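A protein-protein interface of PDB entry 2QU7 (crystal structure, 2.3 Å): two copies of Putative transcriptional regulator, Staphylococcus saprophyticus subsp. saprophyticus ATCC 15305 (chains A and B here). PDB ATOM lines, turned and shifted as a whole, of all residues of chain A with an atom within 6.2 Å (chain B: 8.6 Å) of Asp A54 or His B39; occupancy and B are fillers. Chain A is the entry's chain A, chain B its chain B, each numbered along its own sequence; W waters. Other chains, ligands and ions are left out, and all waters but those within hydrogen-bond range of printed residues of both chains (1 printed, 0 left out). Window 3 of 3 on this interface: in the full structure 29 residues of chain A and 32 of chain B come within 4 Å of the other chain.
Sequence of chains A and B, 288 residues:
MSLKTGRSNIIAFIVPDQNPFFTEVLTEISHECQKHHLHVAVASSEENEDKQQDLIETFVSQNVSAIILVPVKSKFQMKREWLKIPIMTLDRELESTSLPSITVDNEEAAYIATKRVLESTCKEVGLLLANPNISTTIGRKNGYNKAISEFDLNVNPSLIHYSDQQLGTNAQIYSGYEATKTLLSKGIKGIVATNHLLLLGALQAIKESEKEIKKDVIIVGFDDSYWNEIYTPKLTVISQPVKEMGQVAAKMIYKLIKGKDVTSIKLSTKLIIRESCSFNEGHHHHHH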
ATOM      1  N   ALA A  43      -2.303 -14.401 -25.729  1.00  0.00           N
ATOM      2  CA  ALA A  43      -0.962 -14.941 -25.547  1.00  0.00           C
ATOM      3  C   ALA A  43      -0.331 -15.090 -26.936  1.00  0.00           C
ATOM      4  O   ALA A  43      -1.030 -15.382 -27.913  1.00  0.00           O
ATOM      5  CB  ALA A  43      -0.991 -16.269 -24.771  1.00  0.00           C
ATOM      6  N   GLU A  49       5.779 -22.751 -33.513  1.00  0.00           N
ATOM      7  CA  GLU A  49       4.681 -23.729 -33.522  1.00  0.00           C
ATOM      8  C   GLU A  49       4.627 -24.615 -32.282  1.00  0.00           C
ATOM      9  O   GLU A  49       3.547 -25.075 -31.909  1.00  0.00           O
ATOM     10  CB  GLU A  49       4.620 -24.588 -34.797  1.00  0.00           C
ATOM     11  CG  GLU A  49       3.356 -25.497 -34.772  1.00  0.00           C
ATOM     12  CD  GLU A  49       2.864 -26.003 -36.128  1.00  0.00           C
ATOM     13  OE1 GLU A  49       3.643 -26.713 -36.827  1.00  0.00           O
ATOM     14  OE2 GLU A  49       1.674 -25.713 -36.459  1.00  0.00           O
ATOM     15  N   ASP A  50       5.772 -24.860 -31.653  1.00  0.00           N
ATOM     16  CA  ASP A  50       5.770 -25.583 -30.376  1.00  0.00           C
ATOM     17  C   ASP A  50       5.042 -24.740 -29.323  1.00  0.00           C
ATOM     18  O   ASP A  50       4.218 -25.252 -28.565  1.00  0.00           O
ATOM     19  CB  ASP A  50       7.196 -25.870 -29.894  1.00  0.00           C
ATOM     20  CG  ASP A  50       7.875 -26.984 -30.672  1.00  0.00           C
ATOM     21  OD1 ASP A  50       7.214 -27.648 -31.505  1.00  0.00           O
ATOM     22  OD2 ASP A  50       9.086 -27.203 -30.423  1.00  0.00           O
ATOM     23  N   LYS A  51       5.375 -23.450 -29.287  1.00  0.00           N
ATOM     24  CA  LYS A  51       4.790 -22.503 -28.353  1.00  0.00           C
ATOM     25  C   LYS A  51       3.289 -22.432 -28.561  1.00  0.00           C
ATOM     26  O   LYS A  51       2.526 -22.376 -27.596  1.00  0.00           O
ATOM     27  CB  LYS A  51       5.421 -21.111 -28.530  1.00  0.00           C
ATOM     28  CG  LYS A  51       4.831 -20.027 -27.672  1.00  0.00           C
ATOM     29  CD  LYS A  51       4.960 -20.333 -26.198  1.00  0.00           C
ATOM     30  CE  LYS A  51       4.789 -19.066 -25.377  1.00  0.00           C
ATOM     31  NZ  LYS A  51       4.919 -19.368 -23.903  1.00  0.00           N
ATOM     32  N   GLN A  52       2.876 -22.476 -29.828  1.00  0.00           N
ATOM     33  CA  GLN A  52       1.475 -22.371 -30.167  1.00  0.00           C
ATOM     34  C   GLN A  52       0.736 -23.548 -29.561  1.00  0.00           C
ATOM     35  O   GLN A  52      -0.327 -23.365 -28.949  1.00  0.00           O
ATOM     36  CB  GLN A  52       1.289 -22.328 -31.675  1.00  0.00           C
ATOM     37  CG  GLN A  52      -0.149 -22.508 -32.130  1.00  0.00           C
ATOM     38  CD  GLN A  52      -0.310 -22.301 -33.602  1.00  0.00           C
ATOM     39  OE1 GLN A  52      -0.225 -21.168 -34.093  1.00  0.00           O
ATOM     40  NE2 GLN A  52      -0.551 -23.393 -34.334  1.00  0.00           N
ATOM     41  N   GLN A  53       1.326 -24.737 -29.711  1.00  0.00           N
ATOM     42  CA  GLN A  53       0.733 -25.992 -29.276  1.00  0.00           C
ATOM     43  C   GLN A  53       0.605 -26.065 -27.753  1.00  0.00           C
ATOM     44  O   GLN A  53      -0.434 -26.474 -27.231  1.00  0.00           O
ATOM     45  CB  GLN A  53       1.530 -27.174 -29.813  1.00  0.00           C
ATOM     46  CG  GLN A  53       1.163 -28.505 -29.169  1.00  0.00           C
ATOM     47  CD  GLN A  53       1.087 -29.634 -30.176  1.00  0.00           C
ATOM     48  OE1 GLN A  53       0.426 -29.516 -31.223  1.00  0.00           O
ATOM     49  NE2 GLN A  53       1.749 -30.744 -29.867  1.00  0.00           N
ATOM     50  N   ASP A  54       1.666 -25.653 -27.063  1.00  0.00           N
ATOM     51  CA  ASP A  54       1.670 -25.484 -25.620  1.00  0.00           C
ATOM     52  C   ASP A  54       0.545 -24.588 -25.133  1.00  0.00           C
ATOM     53  O   ASP A  54      -0.117 -24.925 -24.175  1.00  0.00           O
ATOM     54  CB  ASP A  54       2.983 -24.864 -25.160  1.00  0.00           C
ATOM     55  CG  ASP A  54       4.124 -25.852 -25.155  1.00  0.00           C
ATOM     56  OD1 ASP A  54       3.914 -27.012 -25.596  1.00  0.00           O
ATOM     57  OD2 ASP A  54       5.236 -25.458 -24.705  1.00  0.00           O
ATOM     58  N   LEU A  55       0.366 -23.440 -25.775  1.00  0.00           N
ATOM     59  CA  LEU A  55      -0.633 -22.474 -25.360  1.00  0.00           C
ATOM     60  C   LEU A  55      -2.024 -23.073 -25.573  1.00  0.00           C
ATOM     61  O   LEU A  55      -2.856 -23.004 -24.678  1.00  0.00           O
ATOM     62  CB  LEU A  55      -0.476 -21.155 -26.125  1.00  0.00           C
ATOM     63  CG  LEU A  55       0.702 -20.232 -25.780  1.00  0.00           C
ATOM     64  CD1 LEU A  55       0.829 -19.096 -26.825  1.00  0.00           C
ATOM     65  CD2 LEU A  55       0.593 -19.643 -24.345  1.00  0.00           C
ATOM     66  N   ILE A  56      -2.258 -23.690 -26.737  1.00  0.00           N
ATOM     67  CA  ILE A  56      -3.526 -24.397 -26.978  1.00  0.00           C
ATOM     68  C   ILE A  56      -3.797 -25.463 -25.902  1.00  0.00           C
ATOM     69  O   ILE A  56      -4.864 -25.455 -25.277  1.00  0.00           O
ATOM     70  CB  ILE A  56      -3.607 -25.032 -28.383  1.00  0.00           C
ATOM     71  CG1 ILE A  56      -3.607 -23.962 -29.467  1.00  0.00           C
ATOM     72  CG2 ILE A  56      -4.872 -25.847 -28.518  1.00  0.00           C
ATOM     73  CD1 ILE A  56      -3.459 -24.541 -30.892  1.00  0.00           C
ATOM     74  N   GLU A  57      -2.819 -26.341 -25.666  1.00  0.00           N
ATOM     75  CA  GLU A  57      -2.912 -27.373 -24.622  1.00  0.00           C
ATOM     76  C   GLU A  57      -3.231 -26.777 -23.241  1.00  0.00           C
ATOM     77  O   GLU A  57      -3.968 -27.358 -22.436  1.00  0.00           O
ATOM     78  CB  GLU A  57      -1.611 -28.209 -24.553  1.00  0.00           C
ATOM     79  CG  GLU A  57      -1.716 -29.640 -25.117  1.00  0.00           C
ATOM     80  CD  GLU A  57      -0.393 -30.167 -25.743  1.00  0.00           C
ATOM     81  OE1 GLU A  57       0.705 -29.950 -25.161  1.00  0.00           O
ATOM     82  OE2 GLU A  57      -0.463 -30.798 -26.826  1.00  0.00           O
ATOM     83  N   THR A  58      -2.643 -25.622 -22.970  1.00  0.00           N
ATOM     84  CA  THR A  58      -2.837 -24.943 -21.704  1.00  0.00           C
ATOM     85  C   THR A  58      -4.267 -24.407 -21.577  1.00  0.00           C
ATOM     86  O   THR A  58      -4.889 -24.529 -20.515  1.00  0.00           O
ATOM     87  CB  THR A  58      -1.796 -23.825 -21.535  1.00  0.00           C
ATOM     88  OG1 THR A  58      -0.501 -24.435 -21.398  1.00  0.00           O
ATOM     89  CG2 THR A  58      -2.108 -22.960 -20.292  1.00  0.00           C
ATOM     90  N   PHE A  59      -4.791 -23.828 -22.652  1.00  0.00           N
ATOM     91  CA  PHE A  59      -6.117 -23.238 -22.578  1.00  0.00           C
ATOM     92  C   PHE A  59      -7.207 -24.310 -22.604  1.00  0.00           C
ATOM     93  O   PHE A  59      -8.242 -24.151 -21.953  1.00  0.00           O
ATOM     94  CB  PHE A  59      -6.315 -22.159 -23.645  1.00  0.00           C
ATOM     95  CG  PHE A  59      -5.490 -20.925 -23.400  1.00  0.00           C
ATOM     96  CD1 PHE A  59      -5.574 -20.240 -22.181  1.00  0.00           C
ATOM     97  CD2 PHE A  59      -4.625 -20.449 -24.369  1.00  0.00           C
ATOM     98  CE1 PHE A  59      -4.796 -19.097 -21.931  1.00  0.00           C
ATOM     99  CE2 PHE A  59      -3.845 -19.295 -24.140  1.00  0.00           C
ATOM    100  CZ  PHE A  59      -3.930 -18.621 -22.922  1.00  0.00           C
ATOM    101  N   SER B   8      -3.203 -23.907 -12.453  1.00  0.00           N
ATOM    102  CA  SER B   8      -3.037 -23.650 -13.883  1.00  0.00           C
ATOM    103  C   SER B   8      -1.629 -23.109 -14.096  1.00  0.00           C
ATOM    104  O   SER B   8      -1.118 -22.395 -13.236  1.00  0.00           O
ATOM    105  CB  SER B   8      -4.080 -22.623 -14.308  1.00  0.00           C
ATOM    106  OG  SER B   8      -3.656 -21.863 -15.408  1.00  0.00           O
ATOM    107  N   ASN B   9      -0.990 -23.454 -15.215  1.00  0.00           N
ATOM    108  CA  ASN B   9       0.360 -22.932 -15.494  1.00  0.00           C
ATOM    109  C   ASN B   9       0.365 -21.552 -16.189  1.00  0.00           C
ATOM    110  O   ASN B   9       1.286 -21.187 -16.925  1.00  0.00           O
ATOM    111  CB  ASN B   9       1.230 -23.969 -16.223  1.00  0.00           C
ATOM    112  CG  ASN B   9       0.713 -24.310 -17.604  1.00  0.00           C
ATOM    113  OD1 ASN B   9      -0.452 -24.081 -17.917  1.00  0.00           O
ATOM    114  ND2 ASN B   9       1.573 -24.889 -18.433  1.00  0.00           N
ATOM    115  N   ILE B  10      -0.687 -20.788 -15.949  1.00  0.00           N
ATOM    116  CA  ILE B  10      -0.825 -19.477 -16.542  1.00  0.00           C
ATOM    117  C   ILE B  10      -0.467 -18.439 -15.515  1.00  0.00           C
ATOM    118  O   ILE B  10      -0.900 -18.537 -14.373  1.00  0.00           O
ATOM    119  CB  ILE B  10      -2.279 -19.220 -16.945  1.00  0.00           C
ATOM    120  CG1 ILE B  10      -2.668 -20.120 -18.095  1.00  0.00           C
ATOM    121  CG2 ILE B  10      -2.504 -17.742 -17.327  1.00  0.00           C
ATOM    122  CD1 ILE B  10      -4.161 -20.157 -18.318  1.00  0.00           C
ATOM    123  N   ILE B  11       0.318 -17.447 -15.923  1.00  0.00           N
ATOM    124  CA  ILE B  11       0.457 -16.213 -15.147  1.00  0.00           C
ATOM    125  C   ILE B  11      -0.349 -15.150 -15.860  1.00  0.00           C
ATOM    126  O   ILE B  11      -0.125 -14.898 -17.035  1.00  0.00           O
ATOM    127  CB  ILE B  11       1.933 -15.786 -14.997  1.00  0.00           C
ATOM    128  CG1 ILE B  11       2.708 -16.861 -14.210  1.00  0.00           C
ATOM    129  CG2 ILE B  11       2.060 -14.365 -14.334  1.00  0.00           C
ATOM    130  CD1 ILE B  11       4.216 -16.709 -14.304  1.00  0.00           C
ATOM    131  N   ALA B  12      -1.311 -14.551 -15.157  1.00  0.00           N
ATOM    132  CA  ALA B  12      -2.176 -13.532 -15.748  1.00  0.00           C
ATOM    133  C   ALA B  12      -1.584 -12.162 -15.506  1.00  0.00           C
ATOM    134  O   ALA B  12      -1.273 -11.805 -14.381  1.00  0.00           O
ATOM    135  CB  ALA B  12      -3.567 -13.615 -15.181  1.00  0.00           C
ATOM    136  N   PHE B  13      -1.390 -11.421 -16.590  1.00  0.00           N
ATOM    137  CA  PHE B  13      -0.788 -10.104 -16.586  1.00  0.00           C
ATOM    138  C   PHE B  13      -1.957  -9.192 -16.933  1.00  0.00           C
ATOM    139  O   PHE B  13      -2.455  -9.240 -18.050  1.00  0.00           O
ATOM    140  CB  PHE B  13       0.312 -10.086 -17.657  1.00  0.00           C
ATOM    141  CG  PHE B  13       1.114  -8.797 -17.758  1.00  0.00           C
ATOM    142  CD1 PHE B  13       1.357  -7.989 -16.653  1.00  0.00           C
ATOM    143  CD2 PHE B  13       1.702  -8.444 -18.984  1.00  0.00           C
ATOM    144  CE1 PHE B  13       2.132  -6.814 -16.780  1.00  0.00           C
ATOM    145  CE2 PHE B  13       2.471  -7.278 -19.127  1.00  0.00           C
ATOM    146  CZ  PHE B  13       2.688  -6.466 -18.021  1.00  0.00           C
ATOM    147  N   LEU B  26       5.898  -7.587 -21.232  1.00  0.00           N
ATOM    148  CA  LEU B  26       5.280  -8.884 -21.351  1.00  0.00           C
ATOM    149  C   LEU B  26       6.229  -9.875 -22.014  1.00  0.00           C
ATOM    150  O   LEU B  26       6.455 -10.961 -21.478  1.00  0.00           O
ATOM    151  CB  LEU B  26       3.957  -8.808 -22.125  1.00  0.00           C
ATOM    152  CG  LEU B  26       3.492 -10.153 -22.722  1.00  0.00           C
ATOM    153  CD1 LEU B  26       3.062 -11.133 -21.637  1.00  0.00           C
ATOM    154  CD2 LEU B  26       2.390 -10.000 -23.746  1.00  0.00           C
ATOM    155  N   ILE B  29       9.044 -10.929 -19.728  1.00  0.00           N
ATOM    156  CA  ILE B  29       8.498 -11.810 -18.685  1.00  0.00           C
ATOM    157  C   ILE B  29       8.259 -13.205 -19.273  1.00  0.00           C
ATOM    158  O   ILE B  29       8.684 -14.219 -18.715  1.00  0.00           O
ATOM    159  CB  ILE B  29       7.176 -11.237 -18.055  1.00  0.00           C
ATOM    160  CG1 ILE B  29       7.487  -9.982 -17.223  1.00  0.00           C
ATOM    161  CG2 ILE B  29       6.466 -12.299 -17.212  1.00  0.00           C
ATOM    162  CD1 ILE B  29       6.283  -9.172 -16.759  1.00  0.00           C
ATOM    163  N   SER B  30       7.602 -13.222 -20.426  1.00  0.00           N
ATOM    164  CA  SER B  30       7.230 -14.446 -21.116  1.00  0.00           C
ATOM    165  C   SER B  30       8.439 -15.328 -21.453  1.00  0.00           C
ATOM    166  O   SER B  30       8.448 -16.513 -21.125  1.00  0.00           O
ATOM    167  CB  SER B  30       6.410 -14.109 -22.356  1.00  0.00           C
ATOM    168  OG  SER B  30       5.935 -15.279 -22.964  1.00  0.00           O
ATOM    169  N   HIS B  31       9.467 -14.737 -22.062  1.00  0.00           N
ATOM    170  CA  HIS B  31      10.713 -15.456 -22.379  1.00  0.00           C
ATOM    171  C   HIS B  31      11.347 -16.133 -21.171  1.00  0.00           C
ATOM    172  O   HIS B  31      11.839 -17.262 -21.277  1.00  0.00           O
ATOM    173  CB  HIS B  31      11.734 -14.526 -23.039  1.00  0.00           C
ATOM    174  CG  HIS B  31      13.056 -15.181 -23.302  1.00  0.00           C
ATOM    175  ND1 HIS B  31      13.279 -15.995 -24.394  1.00  0.00           N
ATOM    176  CD2 HIS B  31      14.220 -15.153 -22.609  1.00  0.00           C
ATOM    177  CE1 HIS B  31      14.524 -16.441 -24.362  1.00  0.00           C
ATOM    178  NE2 HIS B  31      15.118 -15.941 -23.292  1.00  0.00           N
ATOM    179  N   GLU B  32      11.342 -15.455 -20.027  1.00  0.00           N
ATOM    180  CA  GLU B  32      11.933 -16.022 -18.831  1.00  0.00           C
ATOM    181  C   GLU B  32      11.029 -17.072 -18.169  1.00  0.00           C
ATOM    182  O   GLU B  32      11.525 -18.057 -17.632  1.00  0.00           O
ATOM    183  CB  GLU B  32      12.306 -14.916 -17.843  1.00  0.00           C
ATOM    184  CG  GLU B  32      12.936 -15.408 -16.522  1.00  0.00           C
ATOM    185  CD  GLU B  32      14.408 -15.861 -16.633  1.00  0.00           C
ATOM    186  OE1 GLU B  32      15.113 -15.517 -17.633  1.00  0.00           O
ATOM    187  OE2 GLU B  32      14.851 -16.566 -15.689  1.00  0.00           O
ATOM    188  N   CYS B  33       9.714 -16.862 -18.218  1.00  0.00           N
ATOM    189  CA  CYS B  33       8.763 -17.750 -17.543  1.00  0.00           C
ATOM    190  C   CYS B  33       8.611 -19.109 -18.219  1.00  0.00           C
ATOM    191  O   CYS B  33       8.393 -20.122 -17.554  1.00  0.00           O
ATOM    192  CB  CYS B  33       7.400 -17.072 -17.378  1.00  0.00           C
ATOM    193  SG  CYS B  33       7.373 -15.923 -15.975  1.00  0.00           S
ATOM    194  N   GLN B  34       8.732 -19.136 -19.539  1.00  0.00           N
ATOM    195  CA  GLN B  34       8.590 -20.399 -20.242  1.00  0.00           C
ATOM    196  C   GLN B  34       9.705 -21.386 -19.830  1.00  0.00           C
ATOM    197  O   GLN B  34       9.556 -22.593 -20.006  1.00  0.00           O
ATOM    198  CB  GLN B  34       8.382 -20.227 -21.770  1.00  0.00           C
ATOM    199  CG  GLN B  34       9.480 -19.509 -22.561  1.00  0.00           C
ATOM    200  CD  GLN B  34       9.029 -19.106 -23.983  1.00  0.00           C
ATOM    201  OE1 GLN B  34       8.044 -18.380 -24.166  1.00  0.00           O
ATOM    202  NE2 GLN B  34       9.768 -19.559 -24.987  1.00  0.00           N
ATOM    203  N   LYS B  35      10.779 -20.856 -19.231  1.00  0.00           N
ATOM    204  CA  LYS B  35      11.825 -21.662 -18.579  1.00  0.00           C
ATOM    205  C   LYS B  35      11.277 -22.651 -17.545  1.00  0.00           C
ATOM    206  O   LYS B  35      11.790 -23.762 -17.412  1.00  0.00           O
ATOM    207  CB  LYS B  35      12.838 -20.755 -17.877  1.00  0.00           C
ATOM    208  CG  LYS B  35      14.147 -20.514 -18.614  1.00  0.00           C
ATOM    209  CD  LYS B  35      14.059 -19.433 -19.680  1.00  0.00           C
ATOM    210  CE  LYS B  35      15.459 -18.931 -20.078  1.00  0.00           C
ATOM    211  NZ  LYS B  35      16.000 -17.897 -19.111  1.00  0.00           N
ATOM    212  N   HIS B  36      10.264 -22.231 -16.789  1.00  0.00           N
ATOM    213  CA  HIS B  36       9.658 -23.084 -15.763  1.00  0.00           C
ATOM    214  C   HIS B  36       8.323 -23.606 -16.217  1.00  0.00           C
ATOM    215  O   HIS B  36       7.512 -24.005 -15.393  1.00  0.00           O
ATOM    216  CB  HIS B  36       9.481 -22.323 -14.465  1.00  0.00           C
ATOM    217  CG  HIS B  36      10.725 -21.643 -14.002  1.00  0.00           C
ATOM    218  ND1 HIS B  36      10.906 -20.282 -14.101  1.00  0.00           N
ATOM    219  CD2 HIS B  36      11.859 -22.138 -13.453  1.00  0.00           C
ATOM    220  CE1 HIS B  36      12.097 -19.965 -13.625  1.00  0.00           C
ATOM    221  NE2 HIS B  36      12.696 -21.073 -13.226  1.00  0.00           N
ATOM    222  N   HIS B  37       8.108 -23.597 -17.530  1.00  0.00           N
ATOM    223  CA  HIS B  37       6.849 -24.021 -18.140  1.00  0.00           C
ATOM    224  C   HIS B  37       5.636 -23.211 -17.622  1.00  0.00           C
ATOM    225  O   HIS B  37       4.561 -23.748 -17.324  1.00  0.00           O
ATOM    226  CB  HIS B  37       6.690 -25.544 -18.024  1.00  0.00           C
ATOM    227  CG  HIS B  37       7.924 -26.291 -18.427  1.00  0.00           C
ATOM    228  ND1 HIS B  37       8.194 -26.632 -19.737  1.00  0.00           N
ATOM    229  CD2 HIS B  37       8.992 -26.714 -17.701  1.00  0.00           C
ATOM    230  CE1 HIS B  37       9.364 -27.252 -19.797  1.00  0.00           C
ATOM    231  NE2 HIS B  37       9.870 -27.312 -18.575  1.00  0.00           N
ATOM    232  N   LEU B  38       5.840 -21.904 -17.516  1.00  0.00           N
ATOM    233  CA  LEU B  38       4.769 -20.997 -17.200  1.00  0.00           C
ATOM    234  C   LEU B  38       4.511 -20.126 -18.419  1.00  0.00           C
ATOM    235  O   LEU B  38       5.457 -19.582 -19.031  1.00  0.00           O
ATOM    236  CB  LEU B  38       5.102 -20.149 -15.962  1.00  0.00           C
ATOM    237  CG  LEU B  38       5.278 -20.865 -14.612  1.00  0.00           C
ATOM    238  CD1 LEU B  38       6.023 -19.978 -13.620  1.00  0.00           C
ATOM    239  CD2 LEU B  38       3.956 -21.324 -14.026  1.00  0.00           C
ATOM    240  N   HIS B  39       3.232 -20.016 -18.779  1.00  0.00           N
ATOM    241  CA  HIS B  39       2.811 -19.146 -19.867  1.00  0.00           C
ATOM    242  C   HIS B  39       2.199 -17.871 -19.324  1.00  0.00           C
ATOM    243  O   HIS B  39       1.520 -17.892 -18.304  1.00  0.00           O
ATOM    244  CB  HIS B  39       1.789 -19.859 -20.745  1.00  0.00           C
ATOM    245  CG  HIS B  39       2.272 -21.167 -21.274  1.00  0.00           C
ATOM    246  ND1 HIS B  39       3.140 -21.262 -22.344  1.00  0.00           N
ATOM    247  CD2 HIS B  39       2.024 -22.436 -20.874  1.00  0.00           C
ATOM    248  CE1 HIS B  39       3.403 -22.536 -22.577  1.00  0.00           C
ATOM    249  NE2 HIS B  39       2.739 -23.267 -21.699  1.00  0.00           N
ATOM    250  N   VAL B  40       2.408 -16.761 -20.014  1.00  0.00           N
ATOM    251  CA  VAL B  40       1.801 -15.516 -19.609  1.00  0.00           C
ATOM    252  C   VAL B  40       0.600 -15.205 -20.486  1.00  0.00           C
ATOM    253  O   VAL B  40       0.666 -15.303 -21.700  1.00  0.00           O
ATOM    254  CB  VAL B  40       2.800 -14.359 -19.657  1.00  0.00           C
ATOM    255  CG1 VAL B  40       2.198 -13.128 -18.996  1.00  0.00           C
ATOM    256  CG2 VAL B  40       4.128 -14.760 -18.962  1.00  0.00           C
ATOM    257  N   ALA B  41      -0.519 -14.868 -19.874  1.00  0.00           N
ATOM    258  CA  ALA B  41      -1.643 -14.387 -20.650  1.00  0.00           C
ATOM    259  C   ALA B  41      -1.931 -12.950 -20.225  1.00  0.00           C
ATOM    260  O   ALA B  41      -1.780 -12.596 -19.062  1.00  0.00           O
ATOM    261  CB  ALA B  41      -2.852 -15.269 -20.443  1.00  0.00           C
ATOM    262  N   VAL B  42      -2.330 -12.124 -21.172  1.00  0.00           N
ATOM    263  CA  VAL B  42      -2.575 -10.731 -20.874  1.00  0.00           C
ATOM    264  C   VAL B  42      -4.021 -10.400 -21.121  1.00  0.00           C
ATOM    265  O   VAL B  42      -4.593 -10.833 -22.092  1.00  0.00           O
ATOM    266  CB  VAL B  42      -1.660  -9.790 -21.704  1.00  0.00           C
ATOM    267  CG1 VAL B  42      -1.741  -8.356 -21.179  1.00  0.00           C
ATOM    268  CG2 VAL B  42      -0.240 -10.265 -21.608  1.00  0.00           C
ATOM    269  N   VAL B  64      -5.024 -19.571 -11.456  1.00  0.00           N
ATOM    270  CA  VAL B  64      -3.757 -19.318 -12.144  1.00  0.00           C
ATOM    271  C   VAL B  64      -2.597 -19.427 -11.144  1.00  0.00           C
ATOM    272  O   VAL B  64      -2.800 -19.271  -9.932  1.00  0.00           O
ATOM    273  CB  VAL B  64      -3.782 -17.952 -12.876  1.00  0.00           C
ATOM    274  CG1 VAL B  64      -4.964 -17.898 -13.855  1.00  0.00           C
ATOM    275  CG2 VAL B  64      -3.867 -16.793 -11.879  1.00  0.00           C
ATOM    276  N   SER B  65      -1.394 -19.709 -11.647  1.00  0.00           N
ATOM    277  CA  SER B  65      -0.176 -19.693 -10.822  1.00  0.00           C
ATOM    278  C   SER B  65       0.139 -18.342 -10.142  1.00  0.00           C
ATOM    279  O   SER B  65       0.682 -18.315  -9.027  1.00  0.00           O
ATOM    280  CB  SER B  65       1.038 -20.136 -11.630  1.00  0.00           C
ATOM    281  OG  SER B  65       0.951 -21.494 -11.967  1.00  0.00           O
ATOM    282  N   ALA B  66      -0.191 -17.236 -10.803  1.00  0.00           N
ATOM    283  CA  ALA B  66       0.109 -15.900 -10.275  1.00  0.00           C
ATOM    284  C   ALA B  66      -0.591 -14.799 -11.042  1.00  0.00           C
ATOM    285  O   ALA B  66      -1.035 -14.994 -12.169  1.00  0.00           O
ATOM    286  CB  ALA B  66       1.625 -15.640 -10.262  1.00  0.00           C
ATOM    287  N   ILE B 257       5.536 -17.551  -6.348  1.00  0.00           N
ATOM    288  CA  ILE B 257       4.948 -18.857  -6.637  1.00  0.00           C
ATOM    289  C   ILE B 257       5.523 -19.931  -5.716  1.00  0.00           C
ATOM    290  O   ILE B 257       4.808 -20.859  -5.325  1.00  0.00           O
ATOM    291  CB  ILE B 257       5.116 -19.256  -8.117  1.00  0.00           C
ATOM    292  CG1 ILE B 257       4.148 -18.472  -9.003  1.00  0.00           C
ATOM    293  CG2 ILE B 257       4.858 -20.741  -8.315  1.00  0.00           C
ATOM    294  CD1 ILE B 257       4.547 -18.434 -10.459  1.00  0.00           C
HETATM  295  O   HOH W   1       5.593 -17.685 -20.943  1.00  0.00           O
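A ring nitrogen (ND1) of His B39 sits at hydrogen-bond distance from the side-chain amino group of Lys A51 (3.0 Å). A ring nitrogen (NE2) of His B39 lies close to the side-chain hydroxyl (OG1) of Thr A58, at 3.5 Å. The side-chain amino group of Lys A51 sits at hydrogen-bond distance from the side-chain amide oxygen of Gln B34 (3.3 Å). OD1 of Asn B9 lies close to OG1 of Thr A58 (3.5 Å).
No position is printed for both chains. Of the 9 pairs that touch across the chains among the printed residues, none has its exchanged pair printed and touching as well.
Hydrophobic or aromatic side chains of chain A that line the printed part of chain B: Ala A43, Leu A55 and Phe A59. Hydrophobic or aromatic side chains of chain B that line the printed part of chain A: Ile B10 and His B39. Among the printed residues, 9 pairs touch across the chains. Among the printed residues, no Asp or Glu carboxylate lies within 4 Å of a Lys or Arg side-chain nitrogen of the other chain.
Val B40 touches Ala A43 (O to CB, 3.6 Å). His B39 touches Asp A54. Leu A55 touches His B39. CG2 of Thr A58 touches CG1 of Ile B10, at 3.6 Å. Ile B10 touches Phe A59 (CD1 to CE1, 3.8 Å).
Water W1 lies within hydrogen-bond range of the backbone carbonyl oxygen of Leu B38 (2.7 Å), the backbone carbonyl oxygen of Ser B30 (3.1 Å), the backbone NH of Val B40 (3.4 Å) and the side-chain amino group of Lys A51 (3.5 Å).
The side-chain hydroxyl (OG) of Ser B8 sits close to the backbone NH (N) of Ile B10 (3.2 Å). The backbone NH of Ile B11 is in hydrogen-bond range of the backbone carbonyl oxygen of His B39, at 2.7 Å. O of Asn B9 sits at hydrogen-bond distance from N of His B39 (2.9 Å). The backbone NH of Ser B65 is in hydrogen-bond range of the backbone carbonyl oxygen of Ile B10 (3.0 Å). ND2 of Asn B9 lies within hydrogen-bond range of O of His B37 (3.4 Å). O of Asp A54 lies within hydrogen-bond range of OG1 of Thr A58, at 2.8 Å.
Asp A54 touches one residue of chain B. Of chain A, only Lys A51, Asp A54, Leu A55 and Thr A58 come within 4 Å of His B39. Printed residues of chain B within 4 Å of Phe A59: Ile B10 (3.8 Å). Printed residues of chain B within 4 Å of Leu A55: His B39 (3.6 Å). Of the printed residues of chain A, Asn B9 touches Thr A58. Printed residues of chain B within 4 Å of Ala A43: Val B40 (3.6 Å). Of the printed residues of chain B, Lys A51 touches Gln B34 and His B39. Leu B26 touches none of the printed residues of chain A. The nearest printed residue of chain A that does not touch Gln B34 is Asp A54 (6.8 Å).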
